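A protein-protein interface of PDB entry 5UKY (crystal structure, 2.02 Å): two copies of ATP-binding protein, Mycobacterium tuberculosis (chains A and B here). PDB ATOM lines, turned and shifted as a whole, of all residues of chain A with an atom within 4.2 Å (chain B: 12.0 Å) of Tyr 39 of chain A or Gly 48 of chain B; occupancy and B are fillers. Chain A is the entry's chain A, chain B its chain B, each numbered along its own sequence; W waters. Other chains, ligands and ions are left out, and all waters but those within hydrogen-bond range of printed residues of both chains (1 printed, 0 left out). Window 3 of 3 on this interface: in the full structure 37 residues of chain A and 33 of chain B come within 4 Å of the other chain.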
ATOM      1  N   PHE A  35     -25.150 -31.171  29.488  1.00  0.00           N
ATOM      2  CA  PHE A  35     -24.151 -30.289  28.875  1.00  0.00           C
ATOM      3  C   PHE A  35     -24.597 -28.818  28.878  1.00  0.00           C
ATOM      4  O   PHE A  35     -23.794 -27.924  29.135  1.00  0.00           O
ATOM      5  CB  PHE A  35     -23.750 -30.779  27.475  1.00  0.00           C
ATOM      6  CG  PHE A  35     -22.773 -31.955  27.463  1.00  0.00           C
ATOM      7  CD1 PHE A  35     -22.560 -32.750  28.560  1.00  0.00           C
ATOM      8  CD2 PHE A  35     -22.022 -32.222  26.319  1.00  0.00           C
ATOM      9  CE1 PHE A  35     -21.652 -33.819  28.520  1.00  0.00           C
ATOM     10  CE2 PHE A  35     -21.133 -33.312  26.262  1.00  0.00           C
ATOM     11  CZ  PHE A  35     -20.958 -34.101  27.374  1.00  0.00           C
ATOM     12  N   ALA A  36     -25.876 -28.578  28.639  1.00  0.00           N
ATOM     13  CA  ALA A  36     -26.468 -27.219  28.799  1.00  0.00           C
ATOM     14  C   ALA A  36     -26.433 -26.729  30.251  1.00  0.00           C
ATOM     15  O   ALA A  36     -26.100 -25.621  30.480  1.00  0.00           O
ATOM     16  CB  ALA A  36     -27.879 -27.186  28.269  1.00  0.00           C
ATOM     17  N   GLU A  37     -26.727 -27.573  31.216  1.00  0.00           N
ATOM     18  CA  GLU A  37     -26.627 -27.214  32.632  1.00  0.00           C
ATOM     19  C   GLU A  37     -25.154 -26.931  33.032  1.00  0.00           C
ATOM     20  O   GLU A  37     -24.889 -26.046  33.830  1.00  0.00           O
ATOM     21  CB  GLU A  37     -27.236 -28.343  33.490  1.00  0.00           C
ATOM     22  CG  GLU A  37     -27.094 -28.221  35.021  1.00  0.00           C
ATOM     23  CD  GLU A  37     -27.814 -27.009  35.615  1.00  0.00           C
ATOM     24  OE1 GLU A  37     -28.742 -26.465  34.971  1.00  0.00           O
ATOM     25  OE2 GLU A  37     -27.470 -26.589  36.752  1.00  0.00           O
ATOM     26  N   LEU A  38     -24.197 -27.657  32.451  1.00  0.00           N
ATOM     27  CA  LEU A  38     -22.765 -27.380  32.709  1.00  0.00           C
ATOM     28  C   LEU A  38     -22.367 -25.959  32.304  1.00  0.00           C
ATOM     29  O   LEU A  38     -21.649 -25.235  33.035  1.00  0.00           O
ATOM     30  CB  LEU A  38     -21.905 -28.392  31.980  1.00  0.00           C
ATOM     31  CG  LEU A  38     -20.446 -28.568  32.377  1.00  0.00           C
ATOM     32  CD1 LEU A  38     -20.364 -28.982  33.826  1.00  0.00           C
ATOM     33  CD2 LEU A  38     -19.835 -29.711  31.569  1.00  0.00           C
ATOM     34  N   TYR A  39     -22.866 -25.554  31.149  1.00  0.00           N
ATOM     35  CA  TYR A  39     -22.714 -24.190  30.713  1.00  0.00           C
ATOM     36  C   TYR A  39     -23.316 -23.155  31.683  1.00  0.00           C
ATOM     37  O   TYR A  39     -22.718 -22.125  31.979  1.00  0.00           O
ATOM     38  CB  TYR A  39     -23.342 -24.021  29.317  1.00  0.00           C
ATOM     39  CG  TYR A  39     -23.231 -22.614  28.813  1.00  0.00           C
ATOM     40  CD1 TYR A  39     -24.144 -21.637  29.215  1.00  0.00           C
ATOM     41  CD2 TYR A  39     -22.167 -22.232  27.938  1.00  0.00           C
ATOM     42  CE1 TYR A  39     -24.017 -20.308  28.801  1.00  0.00           C
ATOM     43  CE2 TYR A  39     -22.032 -20.903  27.524  1.00  0.00           C
ATOM     44  CZ  TYR A  39     -22.965 -19.937  27.945  1.00  0.00           C
ATOM     45  OH  TYR A  39     -22.845 -18.616  27.501  1.00  0.00           O
ATOM     46  N   ARG A  40     -24.534 -23.376  32.139  1.00  0.00           N
ATOM     47  CA  ARG A  40     -25.202 -22.387  32.992  1.00  0.00           C
ATOM     48  C   ARG A  40     -24.527 -22.278  34.362  1.00  0.00           C
ATOM     49  O   ARG A  40     -24.574 -21.213  34.990  1.00  0.00           O
ATOM     50  CB  ARG A  40     -26.680 -22.784  33.150  1.00  0.00           C
ATOM     51  CG  ARG A  40     -27.548 -21.858  33.964  1.00  0.00           C
ATOM     52  CD  ARG A  40     -29.030 -22.270  33.899  1.00  0.00           C
ATOM     53  NE  ARG A  40     -29.272 -23.379  34.806  1.00  0.00           N
ATOM     54  CZ  ARG A  40     -30.445 -23.732  35.344  1.00  0.00           C
ATOM     55  NH1 ARG A  40     -31.580 -23.072  35.088  1.00  0.00           N
ATOM     56  NH2 ARG A  40     -30.488 -24.773  36.172  1.00  0.00           N
ATOM     57  N   GLN A  41     -23.861 -23.351  34.795  1.00  0.00           N
ATOM     58  CA  GLN A  41     -23.053 -23.356  36.029  1.00  0.00           C
ATOM     59  C   GLN A  41     -21.737 -22.647  35.912  1.00  0.00           C
ATOM     60  O   GLN A  41     -20.978 -22.631  36.860  1.00  0.00           O
ATOM     61  CB  GLN A  41     -22.734 -24.817  36.481  1.00  0.00           C
ATOM     62  CG  GLN A  41     -23.928 -25.592  37.020  1.00  0.00           C
ATOM     63  CD  GLN A  41     -24.547 -24.971  38.265  1.00  0.00           C
ATOM     64  OE1 GLN A  41     -23.847 -24.478  39.167  1.00  0.00           O
ATOM     65  NE2 GLN A  41     -25.880 -24.990  38.317  1.00  0.00           N
ATOM     66  N   GLY A  42     -21.406 -22.119  34.748  1.00  0.00           N
ATOM     67  CA  GLY A  42     -20.152 -21.455  34.564  1.00  0.00           C
ATOM     68  C   GLY A  42     -18.987 -22.348  34.152  1.00  0.00           C
ATOM     69  O   GLY A  42     -17.856 -21.838  34.028  1.00  0.00           O
ATOM     70  N   ALA A  44     -18.042 -24.146  31.342  1.00  0.00           N
ATOM     71  CA  ALA A  44     -17.659 -24.467  29.953  1.00  0.00           C
ATOM     72  C   ALA A  44     -16.541 -23.534  29.482  1.00  0.00           C
ATOM     73  O   ALA A  44     -16.717 -22.294  29.470  1.00  0.00           O
ATOM     74  CB  ALA A  44     -18.827 -24.429  29.009  1.00  0.00           C
ATOM     75  N   VAL A  47     -17.430 -23.990  24.566  1.00  0.00           N
ATOM     76  CA  VAL A  47     -18.798 -24.115  24.169  1.00  0.00           C
ATOM     77  C   VAL A  47     -18.959 -24.704  22.743  1.00  0.00           C
ATOM     78  O   VAL A  47     -19.994 -25.263  22.448  1.00  0.00           O
ATOM     79  CB  VAL A  47     -19.553 -22.751  24.379  1.00  0.00           C
ATOM     80  CG1 VAL A  47     -19.082 -21.688  23.371  1.00  0.00           C
ATOM     81  CG2 VAL A  47     -21.053 -22.956  24.270  1.00  0.00           C
ATOM     82  N   LEU A  50     -18.999 -28.470  23.424  1.00  0.00           N
ATOM     83  CA  LEU A  50     -20.232 -28.721  24.171  1.00  0.00           C
ATOM     84  C   LEU A  50     -21.440 -28.755  23.228  1.00  0.00           C
ATOM     85  O   LEU A  50     -22.247 -29.679  23.246  1.00  0.00           O
ATOM     86  CB  LEU A  50     -20.370 -27.582  25.187  1.00  0.00           C
ATOM     87  CG  LEU A  50     -21.273 -27.660  26.378  1.00  0.00           C
ATOM     88  CD1 LEU A  50     -20.591 -28.524  27.398  1.00  0.00           C
ATOM     89  CD2 LEU A  50     -21.455 -26.285  26.995  1.00  0.00           C
ATOM     90  N   ILE B  32     -33.352 -26.859  17.979  1.00  0.00           N
ATOM     91  CA  ILE B  32     -32.026 -26.866  18.613  1.00  0.00           C
ATOM     92  C   ILE B  32     -30.977 -26.815  17.492  1.00  0.00           C
ATOM     93  O   ILE B  32     -30.004 -26.116  17.602  1.00  0.00           O
ATOM     94  CB  ILE B  32     -31.797 -28.133  19.511  1.00  0.00           C
ATOM     95  CG1 ILE B  32     -32.549 -28.023  20.851  1.00  0.00           C
ATOM     96  CG2 ILE B  32     -30.309 -28.395  19.765  1.00  0.00           C
ATOM     97  CD1 ILE B  32     -32.702 -29.362  21.558  1.00  0.00           C
ATOM     98  N   PHE B  35     -31.185 -23.305  15.564  1.00  0.00           N
ATOM     99  CA  PHE B  35     -30.504 -22.274  16.393  1.00  0.00           C
ATOM    100  C   PHE B  35     -28.997 -22.520  16.448  1.00  0.00           C
ATOM    101  O   PHE B  35     -28.239 -21.573  16.282  1.00  0.00           O
ATOM    102  CB  PHE B  35     -31.084 -22.100  17.814  1.00  0.00           C
ATOM    103  CG  PHE B  35     -32.419 -21.385  17.872  1.00  0.00           C
ATOM    104  CD1 PHE B  35     -33.506 -21.822  17.161  1.00  0.00           C
ATOM    105  CD2 PHE B  35     -32.594 -20.263  18.688  1.00  0.00           C
ATOM    106  CE1 PHE B  35     -34.728 -21.139  17.196  1.00  0.00           C
ATOM    107  CE2 PHE B  35     -33.827 -19.589  18.742  1.00  0.00           C
ATOM    108  CZ  PHE B  35     -34.894 -20.017  17.974  1.00  0.00           C
ATOM    109  N   ALA B  36     -28.556 -23.772  16.678  1.00  0.00           N
ATOM    110  CA  ALA B  36     -27.136 -24.052  16.689  1.00  0.00           C
ATOM    111  C   ALA B  36     -26.463 -23.592  15.388  1.00  0.00           C
ATOM    112  O   ALA B  36     -25.385 -22.957  15.411  1.00  0.00           O
ATOM    113  CB  ALA B  36     -26.909 -25.542  16.889  1.00  0.00           C
ATOM    114  N   LEU B  38     -27.424 -21.277  13.170  1.00  0.00           N
ATOM    115  CA  LEU B  38     -27.428 -19.816  13.099  1.00  0.00           C
ATOM    116  C   LEU B  38     -26.283 -19.211  13.897  1.00  0.00           C
ATOM    117  O   LEU B  38     -25.572 -18.343  13.422  1.00  0.00           O
ATOM    118  CB  LEU B  38     -28.731 -19.305  13.660  1.00  0.00           C
ATOM    119  CG  LEU B  38     -29.272 -17.968  13.261  1.00  0.00           C
ATOM    120  CD1 LEU B  38     -29.623 -17.979  11.773  1.00  0.00           C
ATOM    121  CD2 LEU B  38     -30.525 -17.672  14.068  1.00  0.00           C
ATOM    122  N   TYR B  39     -26.113 -19.702  15.123  1.00  0.00           N
ATOM    123  CA  TYR B  39     -25.036 -19.254  16.012  1.00  0.00           C
ATOM    124  C   TYR B  39     -23.635 -19.608  15.469  1.00  0.00           C
ATOM    125  O   TYR B  39     -22.776 -18.727  15.338  1.00  0.00           O
ATOM    126  CB  TYR B  39     -25.282 -19.735  17.456  1.00  0.00           C
ATOM    127  CG  TYR B  39     -26.222 -18.838  18.249  1.00  0.00           C
ATOM    128  CD1 TYR B  39     -27.602 -18.945  18.158  1.00  0.00           C
ATOM    129  CD2 TYR B  39     -25.732 -17.891  19.070  1.00  0.00           C
ATOM    130  CE1 TYR B  39     -28.443 -18.143  18.918  1.00  0.00           C
ATOM    131  CE2 TYR B  39     -26.563 -17.063  19.807  1.00  0.00           C
ATOM    132  CZ  TYR B  39     -27.929 -17.208  19.750  1.00  0.00           C
ATOM    133  OH  TYR B  39     -28.722 -16.349  20.520  1.00  0.00           O
ATOM    134  N   ARG B  40     -23.460 -20.807  14.974  1.00  0.00           N
ATOM    135  CA  ARG B  40     -22.200 -21.197  14.375  1.00  0.00           C
ATOM    136  C   ARG B  40     -21.839 -20.321  13.168  1.00  0.00           C
ATOM    137  O   ARG B  40     -20.711 -20.088  12.898  1.00  0.00           O
ATOM    138  CB  ARG B  40     -22.215 -22.659  13.973  1.00  0.00           C
ATOM    139  CG  ARG B  40     -22.045 -23.601  15.133  1.00  0.00           C
ATOM    140  CD  ARG B  40     -21.680 -24.994  14.691  1.00  0.00           C
ATOM    141  NE  ARG B  40     -21.711 -25.948  15.776  1.00  0.00           N
ATOM    142  CZ  ARG B  40     -20.737 -26.132  16.646  1.00  0.00           C
ATOM    143  NH1 ARG B  40     -20.865 -27.029  17.588  1.00  0.00           N
ATOM    144  NH2 ARG B  40     -19.641 -25.430  16.575  1.00  0.00           N
ATOM    145  N   ALA B  44     -25.994 -14.660  14.986  1.00  0.00           N
ATOM    146  CA  ALA B  44     -26.674 -14.281  16.219  1.00  0.00           C
ATOM    147  C   ALA B  44     -25.719 -13.932  17.379  1.00  0.00           C
ATOM    148  O   ALA B  44     -24.491 -14.200  17.343  1.00  0.00           O
ATOM    149  CB  ALA B  44     -27.648 -15.376  16.634  1.00  0.00           C
ATOM    150  N   ARG B  45     -26.300 -13.259  18.364  1.00  0.00           N
ATOM    151  CA  ARG B  45     -25.599 -12.853  19.545  1.00  0.00           C
ATOM    152  C   ARG B  45     -26.244 -13.481  20.765  1.00  0.00           C
ATOM    153  O   ARG B  45     -27.439 -13.934  20.749  1.00  0.00           O
ATOM    154  CB  ARG B  45     -25.498 -11.312  19.611  1.00  0.00           C
ATOM    155  CG  ARG B  45     -26.791 -10.577  19.581  1.00  0.00           C
ATOM    156  CD  ARG B  45     -26.601  -9.100  19.901  1.00  0.00           C
ATOM    157  NE  ARG B  45     -25.853  -8.377  18.877  1.00  0.00           N
ATOM    158  CZ  ARG B  45     -26.343  -7.887  17.753  1.00  0.00           C
ATOM    159  NH1 ARG B  45     -25.512  -7.244  16.921  1.00  0.00           N
ATOM    160  NH2 ARG B  45     -27.644  -8.052  17.416  1.00  0.00           N
ATOM    161  N   ASP B  46     -25.420 -13.569  21.802  1.00  0.00           N
ATOM    162  CA  ASP B  46     -25.807 -14.067  23.130  1.00  0.00           C
ATOM    163  C   ASP B  46     -25.933 -15.558  23.210  1.00  0.00           C
ATOM    164  O   ASP B  46     -27.017 -16.164  23.171  1.00  0.00           O
ATOM    165  CB  ASP B  46     -27.070 -13.339  23.633  1.00  0.00           C
ATOM    166  CG  ASP B  46     -27.307 -13.533  25.092  1.00  0.00           C
ATOM    167  OD1 ASP B  46     -26.684 -14.439  25.736  1.00  0.00           O
ATOM    168  OD2 ASP B  46     -28.154 -12.763  25.586  1.00  0.00           O
ATOM    169  N   VAL B  47     -24.778 -16.182  23.307  1.00  0.00           N
ATOM    170  CA  VAL B  47     -24.674 -17.642  23.349  1.00  0.00           C
ATOM    171  C   VAL B  47     -25.367 -18.222  24.579  1.00  0.00           C
ATOM    172  O   VAL B  47     -25.894 -19.340  24.539  1.00  0.00           O
ATOM    173  CB  VAL B  47     -23.196 -18.064  23.310  1.00  0.00           C
ATOM    174  CG1 VAL B  47     -23.052 -19.569  23.390  1.00  0.00           C
ATOM    175  CG2 VAL B  47     -22.507 -17.503  22.062  1.00  0.00           C
ATOM    176  N   GLY B  48     -25.430 -17.434  25.651  1.00  0.00           N
ATOM    177  CA  GLY B  48     -26.194 -17.768  26.843  1.00  0.00           C
ATOM    178  C   GLY B  48     -27.659 -17.978  26.559  1.00  0.00           C
ATOM    179  O   GLY B  48     -28.250 -18.857  27.108  1.00  0.00           O
ATOM    180  N   MET B  49     -28.236 -17.194  25.656  1.00  0.00           N
ATOM    181  CA  MET B  49     -29.607 -17.426  25.173  1.00  0.00           C
ATOM    182  C   MET B  49     -29.748 -18.718  24.343  1.00  0.00           C
ATOM    183  O   MET B  49     -30.775 -19.391  24.384  1.00  0.00           O
ATOM    184  CB  MET B  49     -30.035 -16.222  24.323  1.00  0.00           C
ATOM    185  CG  MET B  49     -31.512 -16.116  23.911  1.00  0.00           C
ATOM    186  SD  MET B  49     -31.848 -14.559  22.982  1.00  0.00           S
ATOM    187  CE  MET B  49     -31.348 -13.321  24.139  1.00  0.00           C
ATOM    188  N   LEU B  50     -28.765 -18.999  23.489  1.00  0.00           N
ATOM    189  CA  LEU B  50     -28.761 -20.250  22.744  1.00  0.00           C
ATOM    190  C   LEU B  50     -28.798 -21.414  23.730  1.00  0.00           C
ATOM    191  O   LEU B  50     -29.675 -22.242  23.647  1.00  0.00           O
ATOM    192  CB  LEU B  50     -27.526 -20.357  21.862  1.00  0.00           C
ATOM    193  CG  LEU B  50     -27.277 -21.697  21.211  1.00  0.00           C
ATOM    194  CD1 LEU B  50     -28.345 -22.000  20.186  1.00  0.00           C
ATOM    195  CD2 LEU B  50     -25.913 -21.704  20.590  1.00  0.00           C
ATOM    196  N   LEU B  51     -27.900 -21.402  24.705  1.00  0.00           N
ATOM    197  CA  LEU B  51     -27.790 -22.538  25.639  1.00  0.00           C
ATOM    198  C   LEU B  51     -29.005 -22.665  26.519  1.00  0.00           C
ATOM    199  O   LEU B  51     -29.420 -23.777  26.766  1.00  0.00           O
ATOM    200  CB  LEU B  51     -26.511 -22.504  26.466  1.00  0.00           C
ATOM    201  CG  LEU B  51     -25.302 -23.235  25.848  1.00  0.00           C
ATOM    202  CD1 LEU B  51     -25.464 -24.762  25.818  1.00  0.00           C
ATOM    203  CD2 LEU B  51     -25.007 -22.762  24.433  1.00  0.00           C
ATOM    204  N   SER B  52     -29.587 -21.534  26.939  1.00  0.00           N
ATOM    205  CA  SER B  52     -30.828 -21.538  27.717  1.00  0.00           C
ATOM    206  C   SER B  52     -32.049 -22.001  26.913  1.00  0.00           C
ATOM    207  O   SER B  52     -32.865 -22.771  27.419  1.00  0.00           O
ATOM    208  CB  SER B  52     -31.024 -20.189  28.447  1.00  0.00           C
ATOM    209  OG  SER B  52     -32.360 -19.774  28.381  1.00  0.00           O
ATOM    210  N   ARG B  53     -32.120 -21.689  25.635  1.00  0.00           N
ATOM    211  CA  ARG B  53     -33.166 -22.207  24.769  1.00  0.00           C
ATOM    212  C   ARG B  53     -33.063 -23.734  24.630  1.00  0.00           C
ATOM    213  O   ARG B  53     -34.041 -24.393  24.596  1.00  0.00           O
ATOM    214  CB  ARG B  53     -33.064 -21.607  23.374  1.00  0.00           C
ATOM    215  CG  ARG B  53     -34.104 -22.096  22.385  1.00  0.00           C
ATOM    216  CD  ARG B  53     -35.479 -21.874  22.962  1.00  0.00           C
ATOM    217  NE  ARG B  53     -36.526 -21.855  21.970  1.00  0.00           N
ATOM    218  CZ  ARG B  53     -36.817 -20.797  21.224  1.00  0.00           C
ATOM    219  NH1 ARG B  53     -36.099 -19.690  21.349  1.00  0.00           N
ATOM    220  NH2 ARG B  53     -37.812 -20.843  20.349  1.00  0.00           N
ATOM    221  N   ILE B  54     -31.847 -24.241  24.501  1.00  0.00           N
ATOM    222  CA  ILE B  54     -31.571 -25.692  24.365  1.00  0.00           C
ATOM    223  C   ILE B  54     -31.987 -26.417  25.665  1.00  0.00           C
ATOM    224  O   ILE B  54     -32.672 -27.462  25.620  1.00  0.00           O
ATOM    225  CB  ILE B  54     -30.076 -25.945  24.022  1.00  0.00           C
ATOM    226  CG1 ILE B  54     -29.774 -25.559  22.574  1.00  0.00           C
ATOM    227  CG2 ILE B  54     -29.700 -27.381  24.260  1.00  0.00           C
ATOM    228  CD1 ILE B  54     -28.273 -25.500  22.229  1.00  0.00           C
ATOM    229  N   GLU B  55     -31.628 -25.825  26.801  1.00  0.00           N
ATOM    230  CA  GLU B  55     -32.047 -26.339  28.136  1.00  0.00           C
ATOM    231  C   GLU B  55     -33.547 -26.416  28.233  1.00  0.00           C
ATOM    232  O   GLU B  55     -34.042 -27.426  28.643  1.00  0.00           O
ATOM    233  CB  GLU B  55     -31.471 -25.491  29.273  1.00  0.00           C
ATOM    234  CG  GLU B  55     -31.200 -26.251  30.543  1.00  0.00           C
ATOM    235  CD  GLU B  55     -30.460 -25.440  31.634  1.00  0.00           C
ATOM    236  OE1 GLU B  55     -29.997 -24.286  31.434  1.00  0.00           O
ATOM    237  OE2 GLU B  55     -30.333 -25.979  32.738  1.00  0.00           O
ATOM    238  N   SER B  56     -34.268 -25.362  27.837  1.00  0.00           N
ATOM    239  CA  SER B  56     -35.752 -25.373  27.837  1.00  0.00           C
ATOM    240  C   SER B  56     -36.403 -26.392  26.920  1.00  0.00           C
ATOM    241  O   SER B  56     -37.385 -27.004  27.284  1.00  0.00           O
ATOM    242  CB  SER B  56     -36.339 -24.030  27.400  1.00  0.00           C
ATOM    243  OG  SER B  56     -36.011 -23.041  28.332  1.00  0.00           O
ATOM    244  N   GLU B  57     -35.914 -26.485  25.699  1.00  0.00           N
ATOM    245  CA  GLU B  57     -36.363 -27.521  24.772  1.00  0.00           C
ATOM    246  C   GLU B  57     -36.088 -28.946  25.330  1.00  0.00           C
ATOM    247  O   GLU B  57     -36.952 -29.833  25.246  1.00  0.00           O
ATOM    248  CB  GLU B  57     -35.683 -27.370  23.396  1.00  0.00           C
ATOM    249  CG  GLU B  57     -35.950 -26.042  22.673  1.00  0.00           C
ATOM    250  CD  GLU B  57     -37.423 -25.724  22.478  1.00  0.00           C
ATOM    251  OE1 GLU B  57     -38.224 -26.651  22.257  1.00  0.00           O
ATOM    252  OE2 GLU B  57     -37.777 -24.540  22.567  1.00  0.00           O
ATOM    253  N   ALA B  58     -34.903 -29.135  25.911  1.00  0.00           N
ATOM    254  CA  ALA B  58     -34.524 -30.440  26.463  1.00  0.00           C
ATOM    255  C   ALA B  58     -35.404 -30.856  27.635  1.00  0.00           C
ATOM    256  O   ALA B  58     -35.791 -32.018  27.734  1.00  0.00           O
ATOM    257  CB  ALA B  58     -33.073 -30.413  26.870  1.00  0.00           C
HETATM  258  O   HOH W   1     -27.747 -23.470  29.825  1.00  0.00           O
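Printed residues of chain B that touch a printed residue of chain A: Val 47, Gly 48, Leu 51 and Glu 55. Hydrophobic or aromatic side chains of chain B within 4 Å of the printed part of chain A: Leu 51.
Water W1 lies within hydrogen-bond range of O of Ala 36 of chain A (2.8 Å) and OE1 of Glu 55 of chain B (2.9 Å).
NE2 of Gln 41 of chain A lies within hydrogen-bond range of OE2 of Glu 37 of chain A (2.7 Å). OD1 of Asp 46 of chain B lies close to N of Gly 48 of chain B (3.2 Å). The side-chain carboxylate (OE1) of Glu 37 of chain A is in salt-bridge range of the guanidinium group (NH2) of Arg 40 of chain A.
Tyr 39 of chain A touches Val 47 of chain B, but with the chains exchanged Val 47 of chain A does not touch Tyr 39 of chain B (8.6 Å).
Of the printed residues of chain B, Ala 36 of chain A touches Leu 51. Of chain B, only Glu 55 (2.8 Å) comes within 4 Å of Glu 37 of chain A. No residue of chain B comes within 4 Å of Leu 38 of chain A. Of the printed residues of chain B, Tyr 39 of chain A touches Val 47, Gly 48 and Leu 51. Of the printed residues of chain B, Arg 40 of chain A touches Glu 55. No residue of chain B comes within 4 Å of Gln 41 of chain A. No residue of chain B comes within 4 Å of Gly 42 of chain A. No residue of chain B comes within 4 Å of Ala 44 of chain A. Val 47 of chain A touches just one residue of chain B: Leu 51 (3.96 Å). Of the printed residues of chain A, Val 47 of chain B touches Tyr 39 (3.9 Å). Gly 48 of chain B touches one residue of chain A. Printed residues of chain A within 4 Å of Leu 51 of chain B: Ala 36 (3.99 Å), Tyr 39 (3.7 Å) and Val 47 (3.96 Å). Printed residues of chain A within 4 Å of Glu 55 of chain B: Glu 37 and Arg 40. The nearest printed residue of chain B that does not touch Tyr 39 of chain A is Met 49 of chain B (5.9 Å). The nearest printed residue of chain A that does not touch Val 47 of chain B is Val 47 of chain A (4.03 Å).
Among the printed residues, merely in contact across the chains: Tyr 39 of chain A with Leu 51 of chain B (3.7 Å), Tyr 39 of chain A with Val 47 of chain B (3.9 Å), Val 47 of chain A with Leu 51 of chain B (3.96 Å) and Ala 36 of chain A with Leu 51 of chain B (3.99 Å).
The side-chain carboxylate (OE1) of Glu 37 of chain A sits close to the side-chain carboxylate (OE2) of Glu 55 of chain B (2.8 Å). The side-chain hydroxyl (OH) of Tyr 39 of chain A is in hydrogen-bond range of the backbone NH (N) of Gly 48 of chain B (3.4 Å). The side-chain carboxylate (OE2) of Glu 55 of chain B is in salt-bridge range of the guanidinium group (NE) of Arg 40 of chain A, at 3.5 Å.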
